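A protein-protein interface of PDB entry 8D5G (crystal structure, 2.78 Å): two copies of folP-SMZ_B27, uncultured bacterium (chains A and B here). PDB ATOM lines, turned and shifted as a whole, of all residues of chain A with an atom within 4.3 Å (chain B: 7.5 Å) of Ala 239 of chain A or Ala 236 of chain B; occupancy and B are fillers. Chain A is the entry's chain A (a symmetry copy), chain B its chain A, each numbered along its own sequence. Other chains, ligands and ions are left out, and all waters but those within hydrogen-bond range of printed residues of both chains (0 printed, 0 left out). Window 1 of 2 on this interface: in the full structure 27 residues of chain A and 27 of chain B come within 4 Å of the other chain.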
ATOM      1  N   ILE A 235     -24.511  17.802  28.059  1.00  0.00           N
ATOM      2  CA  ILE A 235     -24.197  19.216  28.250  1.00  0.00           C
ATOM      3  C   ILE A 235     -23.106  19.646  27.278  1.00  0.00           C
ATOM      4  O   ILE A 235     -23.200  20.699  26.636  1.00  0.00           O
ATOM      5  CB  ILE A 235     -23.794  19.489  29.711  1.00  0.00           C
ATOM      6  CG1 ILE A 235     -24.977  19.245  30.648  1.00  0.00           C
ATOM      7  CG2 ILE A 235     -23.270  20.910  29.869  1.00  0.00           C
ATOM      8  CD1 ILE A 235     -24.601  19.255  32.117  1.00  0.00           C
ATOM      9  N   ALA A 236     -22.059  18.827  27.148  1.00  0.00           N
ATOM     10  CA  ALA A 236     -20.973  19.141  26.228  1.00  0.00           C
ATOM     11  C   ALA A 236     -21.443  19.113  24.779  1.00  0.00           C
ATOM     12  O   ALA A 236     -21.066  19.980  23.981  1.00  0.00           O
ATOM     13  CB  ALA A 236     -19.817  18.164  26.436  1.00  0.00           C
ATOM     14  N   ALA A 237     -22.263  18.122  24.419  1.00  0.00           N
ATOM     15  CA  ALA A 237     -22.752  18.029  23.047  1.00  0.00           C
ATOM     16  C   ALA A 237     -23.663  19.201  22.703  1.00  0.00           C
ATOM     17  O   ALA A 237     -23.587  19.748  21.597  1.00  0.00           O
ATOM     18  CB  ALA A 237     -23.482  16.703  22.836  1.00  0.00           C
ATOM     19  N   SER A 238     -24.527  19.603  23.638  1.00  0.00           N
ATOM     20  CA  SER A 238     -25.419  20.729  23.380  1.00  0.00           C
ATOM     21  C   SER A 238     -24.652  22.044  23.333  1.00  0.00           C
ATOM     22  O   SER A 238     -24.964  22.921  22.519  1.00  0.00           O
ATOM     23  CB  SER A 238     -26.517  20.782  24.440  1.00  0.00           C
ATOM     24  OG  SER A 238     -27.353  19.640  24.363  1.00  0.00           O
ATOM     25  N   ALA A 239     -23.646  22.201  24.196  1.00  0.00           N
ATOM     26  CA  ALA A 239     -22.853  23.426  24.191  1.00  0.00           C
ATOM     27  C   ALA A 239     -22.070  23.569  22.891  1.00  0.00           C
ATOM     28  O   ALA A 239     -22.061  24.640  22.273  1.00  0.00           O
ATOM     29  CB  ALA A 239     -21.912  23.449  25.395  1.00  0.00           C
ATOM     30  N   ILE A 240     -21.403  22.495  22.459  1.00  0.00           N
ATOM     31  CA  ILE A 240     -20.651  22.541  21.208  1.00  0.00           C
ATOM     32  C   ILE A 240     -21.590  22.751  20.027  1.00  0.00           C
ATOM     33  O   ILE A 240     -21.218  23.386  19.030  1.00  0.00           O
ATOM     34  CB  ILE A 240     -19.799  21.263  21.057  1.00  0.00           C
ATOM     35  CG1 ILE A 240     -18.686  21.249  22.108  1.00  0.00           C
ATOM     36  CG2 ILE A 240     -19.200  21.161  19.661  1.00  0.00           C
ATOM     37  CD1 ILE A 240     -17.870  19.977  22.126  1.00  0.00           C
ATOM     38  N   ALA A 241     -22.823  22.249  20.123  1.00  0.00           N
ATOM     39  CA  ALA A 241     -23.803  22.496  19.071  1.00  0.00           C
ATOM     40  C   ALA A 241     -24.156  23.976  18.985  1.00  0.00           C
ATOM     41  O   ALA A 241     -24.245  24.539  17.887  1.00  0.00           O
ATOM     42  CB  ALA A 241     -25.057  21.656  19.310  1.00  0.00           C
ATOM     43  N   VAL A 242     -24.364  24.626  20.133  1.00  0.00           N
ATOM     44  CA  VAL A 242     -24.634  26.060  20.131  1.00  0.00           C
ATOM     45  C   VAL A 242     -23.427  26.825  19.601  1.00  0.00           C
ATOM     46  O   VAL A 242     -23.568  27.812  18.871  1.00  0.00           O
ATOM     47  CB  VAL A 242     -25.035  26.531  21.543  1.00  0.00           C
ATOM     48  CG1 VAL A 242     -25.166  28.048  21.587  1.00  0.00           C
ATOM     49  CG2 VAL A 242     -26.336  25.871  21.967  1.00  0.00           C
ATOM     50  N   LEU A 243     -22.220  26.369  19.950  1.00  0.00           N
ATOM     51  CA  LEU A 243     -21.013  26.999  19.424  1.00  0.00           C
ATOM     52  C   LEU A 243     -20.914  26.849  17.913  1.00  0.00           C
ATOM     53  O   LEU A 243     -20.311  27.696  17.244  1.00  0.00           O
ATOM     54  CB  LEU A 243     -19.773  26.402  20.089  1.00  0.00           C
ATOM     55  CG  LEU A 243     -18.473  27.196  19.928  1.00  0.00           C
ATOM     56  CD1 LEU A 243     -18.284  28.175  21.082  1.00  0.00           C
ATOM     57  CD2 LEU A 243     -17.280  26.259  19.803  1.00  0.00           C
ATOM     58  N   GLY A 260     -25.166  25.247  30.680  1.00  0.00           N
ATOM     59  CA  GLY A 260     -24.006  24.914  29.869  1.00  0.00           C
ATOM     60  C   GLY A 260     -24.001  25.640  28.537  1.00  0.00           C
ATOM     61  O   GLY A 260     -22.965  26.149  28.102  1.00  0.00           O
ATOM     62  N   CYS A 261     -25.158  25.702  27.873  1.00  0.00           N
ATOM     63  CA  CYS A 261     -25.239  26.416  26.603  1.00  0.00           C
ATOM     64  C   CYS A 261     -25.016  27.911  26.786  1.00  0.00           C
ATOM     65  O   CYS A 261     -24.531  28.580  25.865  1.00  0.00           O
ATOM     66  CB  CYS A 261     -26.588  26.151  25.938  1.00  0.00           C
ATOM     67  SG  CYS A 261     -26.767  24.477  25.276  1.00  0.00           S
ATOM     68  N   ALA A 264     -21.487  28.475  26.241  1.00  0.00           N
ATOM     69  CA  ALA A 264     -21.137  28.436  24.825  1.00  0.00           C
ATOM     70  C   ALA A 264     -21.502  29.742  24.129  1.00  0.00           C
ATOM     71  O   ALA A 264     -20.751  30.231  23.276  1.00  0.00           O
ATOM     72  CB  ALA A 264     -21.828  27.254  24.148  1.00  0.00           C
ATOM     73  N   LEU B 196     -10.980  31.450  25.791  1.00  0.00           N
ATOM     74  CA  LEU B 196     -11.484  30.147  25.367  1.00  0.00           C
ATOM     75  C   LEU B 196     -11.856  30.154  23.890  1.00  0.00           C
ATOM     76  O   LEU B 196     -11.643  29.161  23.183  1.00  0.00           O
ATOM     77  CB  LEU B 196     -12.689  29.746  26.217  1.00  0.00           C
ATOM     78  CG  LEU B 196     -12.427  29.358  27.672  1.00  0.00           C
ATOM     79  CD1 LEU B 196     -13.737  29.252  28.438  1.00  0.00           C
ATOM     80  CD2 LEU B 196     -11.657  28.050  27.745  1.00  0.00           C
ATOM     81  N   PRO B 213     -10.796  25.405  33.781  1.00  0.00           N
ATOM     82  CA  PRO B 213     -12.026  26.135  34.114  1.00  0.00           C
ATOM     83  C   PRO B 213     -12.433  25.886  35.559  1.00  0.00           C
ATOM     84  O   PRO B 213     -12.485  26.820  36.360  1.00  0.00           O
ATOM     85  CB  PRO B 213     -13.051  25.574  33.121  1.00  0.00           C
ATOM     86  CG  PRO B 213     -12.222  25.064  31.979  1.00  0.00           C
ATOM     87  CD  PRO B 213     -10.977  24.522  32.616  1.00  0.00           C
ATOM     88  N   LEU B 219     -17.641  31.388  35.398  1.00  0.00           N
ATOM     89  CA  LEU B 219     -18.759  30.508  35.092  1.00  0.00           C
ATOM     90  C   LEU B 219     -19.998  30.821  35.923  1.00  0.00           C
ATOM     91  O   LEU B 219     -20.916  29.996  35.986  1.00  0.00           O
ATOM     92  CB  LEU B 219     -18.350  29.047  35.285  1.00  0.00           C
ATOM     93  CG  LEU B 219     -17.140  28.588  34.472  1.00  0.00           C
ATOM     94  CD1 LEU B 219     -16.649  27.236  34.960  1.00  0.00           C
ATOM     95  CD2 LEU B 219     -17.486  28.536  32.997  1.00  0.00           C
ATOM     96  N   ARG B 230     -21.981  25.340  39.306  1.00  0.00           N
ATOM     97  CA  ARG B 230     -21.134  25.600  38.149  1.00  0.00           C
ATOM     98  C   ARG B 230     -20.675  24.335  37.434  1.00  0.00           C
ATOM     99  O   ARG B 230     -19.883  24.432  36.491  1.00  0.00           O
ATOM    100  CB  ARG B 230     -19.908  26.421  38.566  1.00  0.00           C
ATOM    101  CG  ARG B 230     -20.212  27.870  38.907  1.00  0.00           C
ATOM    102  CD  ARG B 230     -18.993  28.566  39.490  1.00  0.00           C
ATOM    103  NE  ARG B 230     -19.327  29.862  40.069  1.00  0.00           N
ATOM    104  CZ  ARG B 230     -18.533  30.545  40.883  1.00  0.00           C
ATOM    105  NH1 ARG B 230     -17.340  30.090  41.228  1.00  0.00           N
ATOM    106  NH2 ARG B 230     -18.949  31.714  41.363  1.00  0.00           N
ATOM    107  N   LEU B 231     -21.141  23.159  37.854  1.00  0.00           N
ATOM    108  CA  LEU B 231     -20.713  21.930  37.189  1.00  0.00           C
ATOM    109  C   LEU B 231     -21.140  21.857  35.727  1.00  0.00           C
ATOM    110  O   LEU B 231     -20.302  21.469  34.894  1.00  0.00           O
ATOM    111  CB  LEU B 231     -21.214  20.705  37.964  1.00  0.00           C
ATOM    112  CG  LEU B 231     -20.807  19.365  37.343  1.00  0.00           C
ATOM    113  CD1 LEU B 231     -19.294  19.266  37.225  1.00  0.00           C
ATOM    114  CD2 LEU B 231     -21.360  18.198  38.145  1.00  0.00           C
ATOM    115  N   PRO B 232     -22.380  22.186  35.339  1.00  0.00           N
ATOM    116  CA  PRO B 232     -22.681  22.212  33.898  1.00  0.00           C
ATOM    117  C   PRO B 232     -21.810  23.192  33.135  1.00  0.00           C
ATOM    118  O   PRO B 232     -21.354  22.881  32.028  1.00  0.00           O
ATOM    119  CB  PRO B 232     -24.164  22.609  33.858  1.00  0.00           C
ATOM    120  CG  PRO B 232     -24.700  22.177  35.175  1.00  0.00           C
ATOM    121  CD  PRO B 232     -23.590  22.437  36.145  1.00  0.00           C
ATOM    122  N   GLY B 233     -21.554  24.368  33.709  1.00  0.00           N
ATOM    123  CA  GLY B 233     -20.720  25.345  33.030  1.00  0.00           C
ATOM    124  C   GLY B 233     -19.279  24.894  32.888  1.00  0.00           C
ATOM    125  O   GLY B 233     -18.635  25.160  31.869  1.00  0.00           O
ATOM    126  N   THR B 234     -18.752  24.206  33.900  1.00  0.00           N
ATOM    127  CA  THR B 234     -17.377  23.729  33.827  1.00  0.00           C
ATOM    128  C   THR B 234     -17.226  22.533  32.894  1.00  0.00           C
ATOM    129  O   THR B 234     -16.128  22.311  32.371  1.00  0.00           O
ATOM    130  CB  THR B 234     -16.851  23.384  35.226  1.00  0.00           C
ATOM    131  OG1 THR B 234     -15.419  23.411  35.219  1.00  0.00           O
ATOM    132  CG2 THR B 234     -17.312  22.005  35.669  1.00  0.00           C
ATOM    133  N   ILE B 235     -18.296  21.768  32.662  1.00  0.00           N
ATOM    134  CA  ILE B 235     -18.235  20.702  31.665  1.00  0.00           C
ATOM    135  C   ILE B 235     -18.221  21.296  30.263  1.00  0.00           C
ATOM    136  O   ILE B 235     -17.429  20.890  29.405  1.00  0.00           O
ATOM    137  CB  ILE B 235     -19.405  19.719  31.852  1.00  0.00           C
ATOM    138  CG1 ILE B 235     -19.279  18.983  33.186  1.00  0.00           C
ATOM    139  CG2 ILE B 235     -19.465  18.727  30.698  1.00  0.00           C
ATOM    140  CD1 ILE B 235     -20.511  18.179  33.556  1.00  0.00           C
ATOM    141  N   ALA B 236     -19.092  22.278  30.016  1.00  0.00           N
ATOM    142  CA  ALA B 236     -19.143  22.923  28.710  1.00  0.00           C
ATOM    143  C   ALA B 236     -17.866  23.701  28.423  1.00  0.00           C
ATOM    144  O   ALA B 236     -17.348  23.662  27.299  1.00  0.00           O
ATOM    145  CB  ALA B 236     -20.360  23.844  28.633  1.00  0.00           C
ATOM    146  N   ALA B 237     -17.343  24.416  29.423  1.00  0.00           N
ATOM    147  CA  ALA B 237     -16.121  25.187  29.220  1.00  0.00           C
ATOM    148  C   ALA B 237     -14.928  24.278  28.957  1.00  0.00           C
ATOM    149  O   ALA B 237     -14.090  24.578  28.100  1.00  0.00           O
ATOM    150  CB  ALA B 237     -15.857  26.083  30.430  1.00  0.00           C
ATOM    151  N   SER B 238     -14.836  23.160  29.681  1.00  0.00           N
ATOM    152  CA  SER B 238     -13.726  22.236  29.471  1.00  0.00           C
ATOM    153  C   SER B 238     -13.848  21.518  28.133  1.00  0.00           C
ATOM    154  O   SER B 238     -12.841  21.285  27.455  1.00  0.00           O
ATOM    155  CB  SER B 238     -13.655  21.231  30.619  1.00  0.00           C
ATOM    156  OG  SER B 238     -13.353  21.878  31.843  1.00  0.00           O
ATOM    157  N   ALA B 239     -15.072  21.160  27.737  1.00  0.00           N
ATOM    158  CA  ALA B 239     -15.265  20.490  26.455  1.00  0.00           C
ATOM    159  C   ALA B 239     -14.904  21.409  25.294  1.00  0.00           C
ATOM    160  O   ALA B 239     -14.193  21.004  24.367  1.00  0.00           O
ATOM    161  CB  ALA B 239     -16.709  20.002  26.330  1.00  0.00           C
ATOM    162  N   ILE B 240     -15.385  22.654  25.328  1.00  0.00           N
ATOM    163  CA  ILE B 240     -15.062  23.604  24.268  1.00  0.00           C
ATOM    164  C   ILE B 240     -13.569  23.908  24.258  1.00  0.00           C
ATOM    165  O   ILE B 240     -12.983  24.161  23.197  1.00  0.00           O
ATOM    166  CB  ILE B 240     -15.916  24.880  24.424  1.00  0.00           C
ATOM    167  CG1 ILE B 240     -17.387  24.563  24.142  1.00  0.00           C
ATOM    168  CG2 ILE B 240     -15.433  25.986  23.495  1.00  0.00           C
ATOM    169  CD1 ILE B 240     -18.327  25.720  24.390  1.00  0.00           C
ATOM    170  N   ALA B 241     -12.924  23.865  25.427  1.00  0.00           N
ATOM    171  CA  ALA B 241     -11.478  24.050  25.477  1.00  0.00           C
ATOM    172  C   ALA B 241     -10.753  22.914  24.764  1.00  0.00           C
ATOM    173  O   ALA B 241      -9.802  23.151  24.009  1.00  0.00           O
ATOM    174  CB  ALA B 241     -11.010  24.161  26.927  1.00  0.00           C
ATOM    175  N   VAL B 242     -11.185  21.671  24.992  1.00  0.00           N
ATOM    176  CA  VAL B 242     -10.587  20.541  24.288  1.00  0.00           C
ATOM    177  C   VAL B 242     -10.851  20.651  22.791  1.00  0.00           C
ATOM    178  O   VAL B 242      -9.986  20.334  21.966  1.00  0.00           O
ATOM    179  CB  VAL B 242     -11.112  19.213  24.866  1.00  0.00           C
ATOM    180  CG1 VAL B 242     -10.617  18.034  24.038  1.00  0.00           C
ATOM    181  CG2 VAL B 242     -10.683  19.065  26.316  1.00  0.00           C
ATOM    182  N   VAL B 257     -16.079  15.751  33.983  1.00  0.00           N
ATOM    183  CA  VAL B 257     -15.337  16.535  32.998  1.00  0.00           C
ATOM    184  C   VAL B 257     -14.681  15.623  31.967  1.00  0.00           C
ATOM    185  O   VAL B 257     -14.651  15.939  30.771  1.00  0.00           O
ATOM    186  CB  VAL B 257     -14.309  17.442  33.698  1.00  0.00           C
ATOM    187  CG1 VAL B 257     -13.349  18.044  32.686  1.00  0.00           C
ATOM    188  CG2 VAL B 257     -15.018  18.542  34.472  1.00  0.00           C
ATOM    189  N   GLY B 260     -17.452  14.499  29.634  1.00  0.00           N
ATOM    190  CA  GLY B 260     -17.811  15.575  28.724  1.00  0.00           C
ATOM    191  C   GLY B 260     -16.722  15.861  27.707  1.00  0.00           C
ATOM    192  O   GLY B 260     -17.004  16.052  26.521  1.00  0.00           O
ATOM    193  N   CYS B 261     -15.464  15.894  28.153  1.00  0.00           N
ATOM    194  CA  CYS B 261     -14.362  16.126  27.227  1.00  0.00           C
ATOM    195  C   CYS B 261     -14.209  14.980  26.237  1.00  0.00           C
ATOM    196  O   CYS B 261     -13.742  15.193  25.111  1.00  0.00           O
ATOM    197  CB  CYS B 261     -13.063  16.344  28.002  1.00  0.00           C
ATOM    198  SG  CYS B 261     -12.980  17.930  28.868  1.00  0.00           S
ATOM    199  N   ALA B 264     -16.125  15.910  23.317  1.00  0.00           N
ATOM    200  CA  ALA B 264     -15.439  16.910  22.505  1.00  0.00           C
ATOM    201  C   ALA B 264     -14.350  16.274  21.648  1.00  0.00           C
ATOM    202  O   ALA B 264     -14.164  16.654  20.486  1.00  0.00           O
ATOM    203  CB  ALA B 264     -14.850  17.997  23.402  1.00  0.00           C
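Ile 235 of chain A touches Pro 232 of chain B. CB of Ala 236 of chain A touches CB of Ala 239 of chain B, 3.6 Å away. Ala 236 of chain A touches Gly 260 of chain B (CB to O, 3.5 Å). CB of Ala 239 of chain A touches CB of Ala 236 of chain B, 3.6 Å away. Ile 240 of chain A touches Ala 264 of chain B (CD1 to CB, 3.8 Å). Gly 260 of chain A touches Pro 232 of chain B. Gly 260 of chain A touches Ala 236 of chain B. Ala 264 of chain A touches Ile 240 of chain B (CB to CD1, 3.8 Å).
Ala 239 of chain A touches just one residue of chain B: Ala 236. Printed residues of chain A within 4 Å of Ala 236 of chain B: Ala 239 (3.6 Å) and Gly 260 (3.5 Å). Printed residues of chain B within 4 Å of Gly 260 of chain A: Pro 232 (3.98 Å) and Ala 236 (3.5 Å). Of the printed residues of chain A, Pro 232 of chain B touches Ile 235 (3.5 Å) and Gly 260 (3.98 Å). Of the printed residues of chain A, Gly 260 of chain B touches Ala 236. Printed residues of chain A within 4 Å of Ala 239 of chain B: Ala 236. Printed residues of chain A within 4 Å of Ala 264 of chain B: Ile 240 (3.8 Å). Cys 261 of chain B touches none of the printed residues of chain A. The nearest residue of chain B that does not touch Ala 239 of chain A is Ile 240 of chain B (4.4 Å). The nearest printed residue of chain B that does not touch Ile 235 of chain A is Ala 236 of chain B (4.3 Å).
Ala 236 of chain A touches Ala 239 of chain B, and with the chains exchanged Ala 239 of chain A touches Ala 236 of chain B. Ala 236 of chain A touches Gly 260 of chain B, and with the chains exchanged Gly 260 of chain A touches Ala 236 of chain B. Ile 240 of chain A touches Ala 264 of chain B, and with the chains exchanged Ala 264 of chain A touches Ile 240 of chain B. Of the 8 pairs that touch across the chains among the printed residues, 6 have their exchanged pair printed and touching as well.
Printed residues of chain A that touch a printed residue of chain B: Ile 235, Ala 236, Ala 239, Ile 240, Gly 260 and Ala 264. Hydrophobic or aromatic side chains of chain A that line the printed part of chain B: Ile 235, Ala 236, Ala 239, Ile 240 and Ala 264. Of the 20 printed residues of chain B, 6 touch a printed residue of chain A. Hydrophobic or aromatic side chains of chain B that line the printed part of chain A: Pro 232, Ala 236, Ala 239, Ile 240 and Ala 264. Among the printed residues, 8 pairs touch across the chains. Among the printed residues, no Asp or Glu carboxylate lies within 4 Å of a Lys or Arg side-chain nitrogen of the other chain.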
